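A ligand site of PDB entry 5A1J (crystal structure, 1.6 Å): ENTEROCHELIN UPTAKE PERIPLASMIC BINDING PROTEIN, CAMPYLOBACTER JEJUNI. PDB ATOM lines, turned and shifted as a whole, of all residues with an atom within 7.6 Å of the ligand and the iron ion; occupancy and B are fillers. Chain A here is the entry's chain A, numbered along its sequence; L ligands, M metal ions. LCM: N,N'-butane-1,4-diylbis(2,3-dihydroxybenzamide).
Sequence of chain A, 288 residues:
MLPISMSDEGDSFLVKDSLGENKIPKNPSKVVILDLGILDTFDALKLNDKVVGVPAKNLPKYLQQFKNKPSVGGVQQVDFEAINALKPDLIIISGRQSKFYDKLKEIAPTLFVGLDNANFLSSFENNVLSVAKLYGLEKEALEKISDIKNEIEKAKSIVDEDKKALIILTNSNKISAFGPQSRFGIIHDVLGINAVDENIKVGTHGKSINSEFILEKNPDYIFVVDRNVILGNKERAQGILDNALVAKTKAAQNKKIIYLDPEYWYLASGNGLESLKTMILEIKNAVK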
ATOM      1  N   LYS A  57      25.616 -17.561   6.484  1.00  0.00           N
ATOM      2  CA  LYS A  57      25.963 -17.420   5.041  1.00  0.00           C
ATOM      3  C   LYS A  57      26.570 -16.052   4.731  1.00  0.00           C
ATOM      4  O   LYS A  57      27.444 -15.930   3.886  1.00  0.00           O
ATOM      5  CB  LYS A  57      24.703 -17.519   4.202  1.00  0.00           C
ATOM      6  CG  LYS A  57      24.942 -17.178   2.706  1.00  0.00           C
ATOM      7  CD  LYS A  57      23.931 -17.936   1.870  1.00  0.00           C
ATOM      8  CE  LYS A  57      24.132 -17.741   0.368  1.00  0.00           C
ATOM      9  NZ  LYS A  57      23.313 -16.656  -0.241  1.00  0.00           N
ATOM     10  N   ASN A  58      25.962 -15.049   5.362  1.00  0.00           N
ATOM     11  CA  ASN A  58      26.303 -13.678   5.233  1.00  0.00           C
ATOM     12  C   ASN A  58      26.760 -13.159   6.604  1.00  0.00           C
ATOM     13  O   ASN A  58      26.171 -12.198   7.099  1.00  0.00           O
ATOM     14  CB  ASN A  58      25.055 -12.872   4.751  1.00  0.00           C
ATOM     15  CG  ASN A  58      24.477 -13.367   3.426  1.00  0.00           C
ATOM     16  OD1 ASN A  58      23.306 -13.768   3.327  1.00  0.00           O
ATOM     17  ND2 ASN A  58      25.314 -13.363   2.396  1.00  0.00           N
ATOM     18  N   GLY A  74      20.858 -17.143   5.146  1.00  0.00           N
ATOM     19  CA  GLY A  74      21.281 -15.850   4.571  1.00  0.00           C
ATOM     20  C   GLY A  74      20.023 -14.960   4.499  1.00  0.00           C
ATOM     21  O   GLY A  74      18.973 -15.349   4.949  1.00  0.00           O
ATOM     22  N   VAL A  75      20.092 -13.776   3.882  1.00  0.00           N
ATOM     23  CA  VAL A  75      19.045 -12.750   4.013  1.00  0.00           C
ATOM     24  C   VAL A  75      17.846 -12.767   2.982  1.00  0.00           C
ATOM     25  O   VAL A  75      16.793 -12.128   3.196  1.00  0.00           O
ATOM     26  CB  VAL A  75      19.710 -11.360   4.039  1.00  0.00           C
ATOM     27  CG1 VAL A  75      20.745 -11.246   5.161  1.00  0.00           C
ATOM     28  CG2 VAL A  75      20.333 -11.101   2.673  1.00  0.00           C
ATOM     29  N   GLN A  76      18.015 -13.423   1.834  1.00  0.00           N
ATOM     30  CA  GLN A  76      16.835 -13.847   1.026  1.00  0.00           C
ATOM     31  C   GLN A  76      16.935 -15.332   0.719  1.00  0.00           C
ATOM     32  O   GLN A  76      16.315 -15.800  -0.240  1.00  0.00           O
ATOM     33  CB  GLN A  76      16.636 -13.058  -0.293  1.00  0.00           C
ATOM     34  CG  GLN A  76      16.570 -11.511  -0.211  1.00  0.00           C
ATOM     35  CD  GLN A  76      17.846 -10.901  -0.753  1.00  0.00           C
ATOM     36  OE1 GLN A  76      18.124  -9.703  -0.622  1.00  0.00           O
ATOM     37  NE2 GLN A  76      18.646 -11.766  -1.356  1.00  0.00           N
ATOM     38  N   GLN A  77      17.753 -16.055   1.488  1.00  0.00           N
ATOM     39  CA  GLN A  77      17.699 -17.508   1.585  1.00  0.00           C
ATOM     40  C   GLN A  77      17.636 -17.839   3.079  1.00  0.00           C
ATOM     41  O   GLN A  77      18.497 -18.528   3.679  1.00  0.00           O
ATOM     42  CB  GLN A  77      18.895 -18.178   0.975  1.00  0.00           C
ATOM     43  CG  GLN A  77      18.889 -19.673   1.211  1.00  0.00           C
ATOM     44  CD  GLN A  77      19.580 -20.410   0.117  1.00  0.00           C
ATOM     45  OE1 GLN A  77      19.233 -20.265  -1.049  1.00  0.00           O
ATOM     46  NE2 GLN A  77      20.567 -21.214   0.489  1.00  0.00           N
ATOM     47  N   SER A  94      14.218  -6.700   8.314  1.00  0.00           N
ATOM     48  CA  SER A  94      14.188  -5.438   7.577  1.00  0.00           C
ATOM     49  C   SER A  94      13.783  -5.722   6.138  1.00  0.00           C
ATOM     50  O   SER A  94      13.091  -6.700   5.840  1.00  0.00           O
ATOM     51  CB  SER A  94      15.569  -4.697   7.682  1.00  0.00           C
ATOM     52  OG  SER A  94      16.607  -5.458   7.167  1.00  0.00           O
ATOM     53  N   GLY A  95      14.160  -4.844   5.239  1.00  0.00           N
ATOM     54  CA  GLY A  95      13.529  -4.787   3.967  1.00  0.00           C
ATOM     55  C   GLY A  95      13.606  -5.995   3.093  1.00  0.00           C
ATOM     56  O   GLY A  95      12.689  -6.269   2.298  1.00  0.00           O
ATOM     57  N   ARG A  96      14.689  -6.762   3.285  1.00  0.00           N
ATOM     58  CA  ARG A  96      14.954  -7.914   2.427  1.00  0.00           C
ATOM     59  C   ARG A  96      14.056  -9.105   2.766  1.00  0.00           C
ATOM     60  O   ARG A  96      14.069 -10.095   2.033  1.00  0.00           O
ATOM     61  CB  ARG A  96      16.406  -8.339   2.539  1.00  0.00           C
ATOM     62  CG  ARG A  96      17.465  -7.518   1.826  1.00  0.00           C
ATOM     63  CD  ARG A  96      18.771  -8.236   2.109  1.00  0.00           C
ATOM     64  NE  ARG A  96      19.926  -7.835   1.322  1.00  0.00           N
ATOM     65  CZ  ARG A  96      20.818  -6.946   1.689  1.00  0.00           C
ATOM     66  NH1 ARG A  96      20.703  -6.343   2.876  1.00  0.00           N
ATOM     67  NH2 ARG A  96      21.851  -6.615   0.908  1.00  0.00           N
ATOM     68  N   GLN A  97      13.329  -9.015   3.889  1.00  0.00           N
ATOM     69  CA  GLN A  97      12.432 -10.128   4.297  1.00  0.00           C
ATOM     70  C   GLN A  97      10.991  -9.749   4.384  1.00  0.00           C
ATOM     71  O   GLN A  97      10.171 -10.614   4.692  1.00  0.00           O
ATOM     72  CB  GLN A  97      12.808 -10.707   5.643  1.00  0.00           C
ATOM     73  CG  GLN A  97      14.165 -11.347   5.720  1.00  0.00           C
ATOM     74  CD  GLN A  97      15.180 -10.298   6.000  1.00  0.00           C
ATOM     75  OE1 GLN A  97      14.822  -9.300   6.615  1.00  0.00           O
ATOM     76  NE2 GLN A  97      16.448 -10.513   5.618  1.00  0.00           N
ATOM     77  N   SER A  98      10.672  -8.501   4.143  1.00  0.00           N
ATOM     78  CA  SER A  98       9.330  -7.968   4.210  1.00  0.00           C
ATOM     79  C   SER A  98       8.311  -8.819   3.484  1.00  0.00           C
ATOM     80  O   SER A  98       7.149  -8.915   3.879  1.00  0.00           O
ATOM     81  CB  SER A  98       9.345  -6.572   3.592  1.00  0.00           C
ATOM     82  OG  SER A  98      10.042  -5.689   4.425  1.00  0.00           O
ATOM     83  N   LYS A  99       8.749  -9.417   2.381  1.00  0.00           N
ATOM     84  CA  LYS A  99       7.910 -10.319   1.611  1.00  0.00           C
ATOM     85  C   LYS A  99       7.494 -11.605   2.391  1.00  0.00           C
ATOM     86  O   LYS A  99       6.414 -12.138   2.095  1.00  0.00           O
ATOM     87  CB  LYS A  99       8.574 -10.620   0.251  1.00  0.00           C
ATOM     88  CG  LYS A  99       9.828 -11.503   0.316  1.00  0.00           C
ATOM     89  CD  LYS A  99      10.719 -11.563  -0.930  1.00  0.00           C
ATOM     90  CE  LYS A  99      11.975 -12.395  -0.603  1.00  0.00           C
ATOM     91  NZ  LYS A  99      13.231 -12.140  -1.360  1.00  0.00           N
ATOM     92  N   LEU A 169      27.645   0.777  -7.670  1.00  0.00           N
ATOM     93  CA  LEU A 169      27.711  -0.628  -7.279  1.00  0.00           C
ATOM     94  C   LEU A 169      28.191  -1.402  -8.417  1.00  0.00           C
ATOM     95  O   LEU A 169      27.839  -1.116  -9.572  1.00  0.00           O
ATOM     96  CB  LEU A 169      26.302  -1.055  -6.979  1.00  0.00           C
ATOM     97  CG  LEU A 169      25.979  -2.440  -6.440  1.00  0.00           C
ATOM     98  CD1 LEU A 169      25.239  -2.312  -5.146  1.00  0.00           C
ATOM     99  CD2 LEU A 169      25.236  -3.329  -7.410  1.00  0.00           C
ATOM    100  N   ARG A 183      19.916   3.802  -0.843  1.00  0.00           N
ATOM    101  CA  ARG A 183      20.378   2.938   0.247  1.00  0.00           C
ATOM    102  C   ARG A 183      21.815   3.261   0.765  1.00  0.00           C
ATOM    103  O   ARG A 183      22.275   2.666   1.862  1.00  0.00           O
ATOM    104  CB  ARG A 183      20.420   1.465  -0.218  1.00  0.00           C
ATOM    105  CG  ARG A 183      21.432   1.122  -1.276  1.00  0.00           C
ATOM    106  CD  ARG A 183      21.098  -0.272  -1.822  1.00  0.00           C
ATOM    107  NE  ARG A 183      21.234  -1.366  -0.765  1.00  0.00           N
ATOM    108  CZ  ARG A 183      20.901  -2.654  -1.002  1.00  0.00           C
ATOM    109  NH1 ARG A 183      20.455  -3.132  -2.182  1.00  0.00           N
ATOM    110  NH2 ARG A 183      21.085  -3.532  -0.041  1.00  0.00           N
ATOM    111  N   THR A 204      16.480   0.043  -5.699  1.00  0.00           N
ATOM    112  CA  THR A 204      17.072  -0.872  -4.697  1.00  0.00           C
ATOM    113  C   THR A 204      18.432  -1.366  -5.143  1.00  0.00           C
ATOM    114  O   THR A 204      19.346  -1.476  -4.323  1.00  0.00           O
ATOM    115  CB  THR A 204      16.155  -2.071  -4.470  1.00  0.00           C
ATOM    116  OG1 THR A 204      14.927  -1.665  -3.856  1.00  0.00           O
ATOM    117  CG2 THR A 204      16.872  -3.024  -3.543  1.00  0.00           C
ATOM    118  N   HIS A 205      18.604  -1.667  -6.444  1.00  0.00           N
ATOM    119  CA  HIS A 205      19.919  -2.023  -6.961  1.00  0.00           C
ATOM    120  C   HIS A 205      20.519  -1.028  -7.955  1.00  0.00           C
ATOM    121  O   HIS A 205      21.522  -1.247  -8.610  1.00  0.00           O
ATOM    122  CB  HIS A 205      19.928  -3.456  -7.445  1.00  0.00           C
ATOM    123  CG  HIS A 205      19.689  -4.474  -6.356  1.00  0.00           C
ATOM    124  ND1 HIS A 205      18.488  -5.049  -6.099  1.00  0.00           N
ATOM    125  CD2 HIS A 205      20.549  -4.963  -5.448  1.00  0.00           C
ATOM    126  CE1 HIS A 205      18.598  -5.933  -5.118  1.00  0.00           C
ATOM    127  NE2 HIS A 205      19.832  -5.863  -4.666  1.00  0.00           N
ATOM    128  N   ARG A 227      29.171  -5.604  -5.088  1.00  0.00           N
ATOM    129  CA  ARG A 227      28.110  -6.568  -4.763  1.00  0.00           C
ATOM    130  C   ARG A 227      28.570  -7.997  -5.019  1.00  0.00           C
ATOM    131  O   ARG A 227      27.956  -8.982  -4.528  1.00  0.00           O
ATOM    132  CB  ARG A 227      26.777  -6.207  -5.431  1.00  0.00           C
ATOM    133  CG  ARG A 227      25.692  -7.278  -5.213  1.00  0.00           C
ATOM    134  CD  ARG A 227      24.357  -6.754  -5.750  1.00  0.00           C
ATOM    135  NE  ARG A 227      23.245  -7.654  -5.585  1.00  0.00           N
ATOM    136  CZ  ARG A 227      22.929  -8.676  -6.378  1.00  0.00           C
ATOM    137  NH1 ARG A 227      23.617  -8.970  -7.485  1.00  0.00           N
ATOM    138  NH2 ARG A 227      21.888  -9.400  -6.083  1.00  0.00           N
ATOM    139  N   ILE A 230      29.547 -10.197  -1.678  1.00  0.00           N
ATOM    140  CA  ILE A 230      28.407 -10.685  -0.961  1.00  0.00           C
ATOM    141  C   ILE A 230      27.775 -11.887  -1.663  1.00  0.00           C
ATOM    142  O   ILE A 230      27.482 -12.893  -1.023  1.00  0.00           O
ATOM    143  CB  ILE A 230      27.365  -9.544  -0.862  1.00  0.00           C
ATOM    144  CG1 ILE A 230      27.982  -8.261  -0.225  1.00  0.00           C
ATOM    145  CG2 ILE A 230      26.101 -10.016  -0.176  1.00  0.00           C
ATOM    146  CD1 ILE A 230      28.960  -8.495   0.913  1.00  0.00           C
ATOM    147  N   LEU A 231      27.636 -11.783  -2.981  1.00  0.00           N
ATOM    148  CA  LEU A 231      26.853 -12.695  -3.805  1.00  0.00           C
ATOM    149  C   LEU A 231      27.640 -13.854  -4.356  1.00  0.00           C
ATOM    150  O   LEU A 231      27.030 -14.771  -4.862  1.00  0.00           O
ATOM    151  CB  LEU A 231      26.192 -11.940  -4.953  1.00  0.00           C
ATOM    152  CG  LEU A 231      24.745 -11.413  -4.847  1.00  0.00           C
ATOM    153  CD1 LEU A 231      23.718 -12.501  -5.111  1.00  0.00           C
ATOM    154  CD2 LEU A 231      24.478 -10.685  -3.522  1.00  0.00           C
ATOM    155  N   TYR A 266      26.461  -2.768   1.887  1.00  0.00           N
ATOM    156  CA  TYR A 266      25.459  -3.557   1.193  1.00  0.00           C
ATOM    157  C   TYR A 266      24.649  -4.522   2.057  1.00  0.00           C
ATOM    158  O   TYR A 266      23.426  -4.703   1.907  1.00  0.00           O
ATOM    159  CB  TYR A 266      26.102  -4.406   0.057  1.00  0.00           C
ATOM    160  CG  TYR A 266      25.042  -4.933  -0.866  1.00  0.00           C
ATOM    161  CD1 TYR A 266      24.317  -4.091  -1.669  1.00  0.00           C
ATOM    162  CD2 TYR A 266      24.708  -6.289  -0.916  1.00  0.00           C
ATOM    163  CE1 TYR A 266      23.294  -4.578  -2.476  1.00  0.00           C
ATOM    164  CE2 TYR A 266      23.728  -6.817  -1.726  1.00  0.00           C
ATOM    165  CZ  TYR A 266      22.964  -5.940  -2.519  1.00  0.00           C
ATOM    166  OH  TYR A 266      21.919  -6.399  -3.289  1.00  0.00           O
ATOM    167  N   LEU A 267      25.400  -5.257   2.883  1.00  0.00           N
ATOM    168  CA  LEU A 267      24.791  -6.136   3.825  1.00  0.00           C
ATOM    169  C   LEU A 267      24.173  -5.330   4.981  1.00  0.00           C
ATOM    170  O   LEU A 267      22.951  -5.188   5.027  1.00  0.00           O
ATOM    171  CB  LEU A 267      25.789  -7.237   4.247  1.00  0.00           C
ATOM    172  CG  LEU A 267      26.147  -8.477   3.419  1.00  0.00           C
ATOM    173  CD1 LEU A 267      26.981  -9.408   4.285  1.00  0.00           C
ATOM    174  CD2 LEU A 267      24.911  -9.208   3.023  1.00  0.00           C
ATOM    175  N   SER A 269      23.994  -2.241   5.831  1.00  0.00           N
ATOM    176  CA  SER A 269      23.189  -1.135   5.348  1.00  0.00           C
ATOM    177  C   SER A 269      23.224   0.001   6.384  1.00  0.00           C
ATOM    178  O   SER A 269      22.325   0.834   6.437  1.00  0.00           O
ATOM    179  CB  SER A 269      21.757  -1.610   4.998  1.00  0.00           C
ATOM    180  OG  SER A 269      21.747  -2.826   4.225  1.00  0.00           O
HETATM  181  C1  LCM L   1      21.754 -10.420  -0.691  1.00  0.00           C
HETATM  182  C2  LCM L   1      21.293  -9.479  -1.613  1.00  0.00           C
HETATM  183  C3  LCM L   1      20.781  -9.933  -2.866  1.00  0.00           C
HETATM  184  C4  LCM L   1      20.868 -11.361  -3.231  1.00  0.00           C
HETATM  185  C5  LCM L   1      21.414 -12.266  -2.296  1.00  0.00           C
HETATM  186  C6  LCM L   1      21.817 -11.780  -1.054  1.00  0.00           C
HETATM  187  C7  LCM L   1      20.250 -11.750  -4.526  1.00  0.00           C
HETATM  188  N8  LCM L   1      19.465 -10.776  -5.050  1.00  0.00           N
HETATM  189  O9  LCM L   1      20.194 -12.934  -4.841  1.00  0.00           O
HETATM  190  C10 LCM L   1      18.172 -10.967  -5.691  1.00  0.00           C
HETATM  191  C11 LCM L   1      17.208 -11.231  -4.471  1.00  0.00           C
HETATM  192  C12 LCM L   1      15.759 -10.890  -4.744  1.00  0.00           C
HETATM  193  C13 LCM L   1      15.086  -9.966  -3.728  1.00  0.00           C
HETATM  194  N14 LCM L   1      15.931  -8.898  -3.163  1.00  0.00           N
HETATM  195  C15 LCM L   1      15.401  -7.921  -2.353  1.00  0.00           C
HETATM  196  C16 LCM L   1      16.220  -6.829  -1.694  1.00  0.00           C
HETATM  197  O17 LCM L   1      14.204  -7.904  -2.157  1.00  0.00           O
HETATM  198  C18 LCM L   1      17.697  -6.725  -1.970  1.00  0.00           C
HETATM  199  C19 LCM L   1      18.464  -5.683  -1.297  1.00  0.00           C
HETATM  200  C20 LCM L   1      17.793  -4.811  -0.415  1.00  0.00           C
HETATM  201  C21 LCM L   1      16.436  -4.893  -0.187  1.00  0.00           C
HETATM  202  C22 LCM L   1      15.651  -5.873  -0.824  1.00  0.00           C
HETATM  203  O23 LCM L   1      18.432  -7.669  -2.707  1.00  0.00           O
HETATM  204  O24 LCM L   1      19.760  -5.733  -1.679  1.00  0.00           O
HETATM  205  O25 LCM L   1      20.336  -9.009  -3.726  1.00  0.00           O
HETATM  206  O26 LCM L   1      21.139  -8.229  -1.252  1.00  0.00           O
HETATM  207 FE    FE M   1      20.266  -7.073  -2.867  1.00  0.00          FE
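The guanidinium group (NH1) of Arg 183 lies close to an oxygen (O24) of the ligand.
The guanidinium group of Arg 96 lies close to an oxygen (O26) of the ligand (2.8 Å).
NH2 of Arg 227 sits close to O25 of the ligand.
A nitrogen (N14) of the ligand sits close to the side-chain amide oxygen (OE1) of Gln 76 (3.5 Å).
Of the 22 residues printed, 2 come within 4 Å of the iron ion.
The nearest printed residue that does not touch the iron ion is Arg 183 (4.005 Å).
Val 75 touches the ligand.
Lys 99 touches the ligand.
Thr 204 touches the ligand (CG2 to C20, 3.7 Å).
Leu 231 touches the ligand (CD1 to O9, 3.6 Å).
Hydrophobic or aromatic side chains that line the ligand: Val 75, His 205, Leu 231 and Tyr 266.
The nearest printed residue that does not touch the ligand is Gly 95 (4.3 Å).
O of Tyr 266 sits at hydrogen-bond distance from NH2 of Arg 183 (3.3 Å).
The guanidinium group of Arg 96 is in hydrogen-bond range of the backbone carbonyl oxygen of Tyr 266 (2.7 Å).
The side-chain hydroxyl (OH) of Tyr 266 sits close to the guanidinium group (NE) of Arg 227 (2.9 Å).
O of Thr 204 lies within hydrogen-bond range of NH1 of Arg 183, at 2.9 Å.
The guanidinium group (NE) of Arg 96 lies close to the side-chain amide oxygen (OE1) of Gln 76, 3.2 Å away.
The guanidinium group (NH1) of Arg 96 is in hydrogen-bond range of the backbone carbonyl oxygen (O) of Leu 267, 3.3 Å away.
The backbone NH (N) of Val 75 sits at hydrogen-bond distance from the side-chain amide oxygen (OD1) of Asn 58.
The backbone carbonyl oxygen (O) of Val 75 lies within hydrogen-bond range of the side-chain amide nitrogen (NE2) of Gln 97 (2.9 Å).
The iron ion is bound by the side-chain hydroxyl (OH) of Tyr 266, an oxygen (O24) of the ligand, an oxygen (O23) of the ligand, an oxygen (O25) of the ligand, an oxygen (O26) of the ligand and a ring nitrogen (NE2) of His 205.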
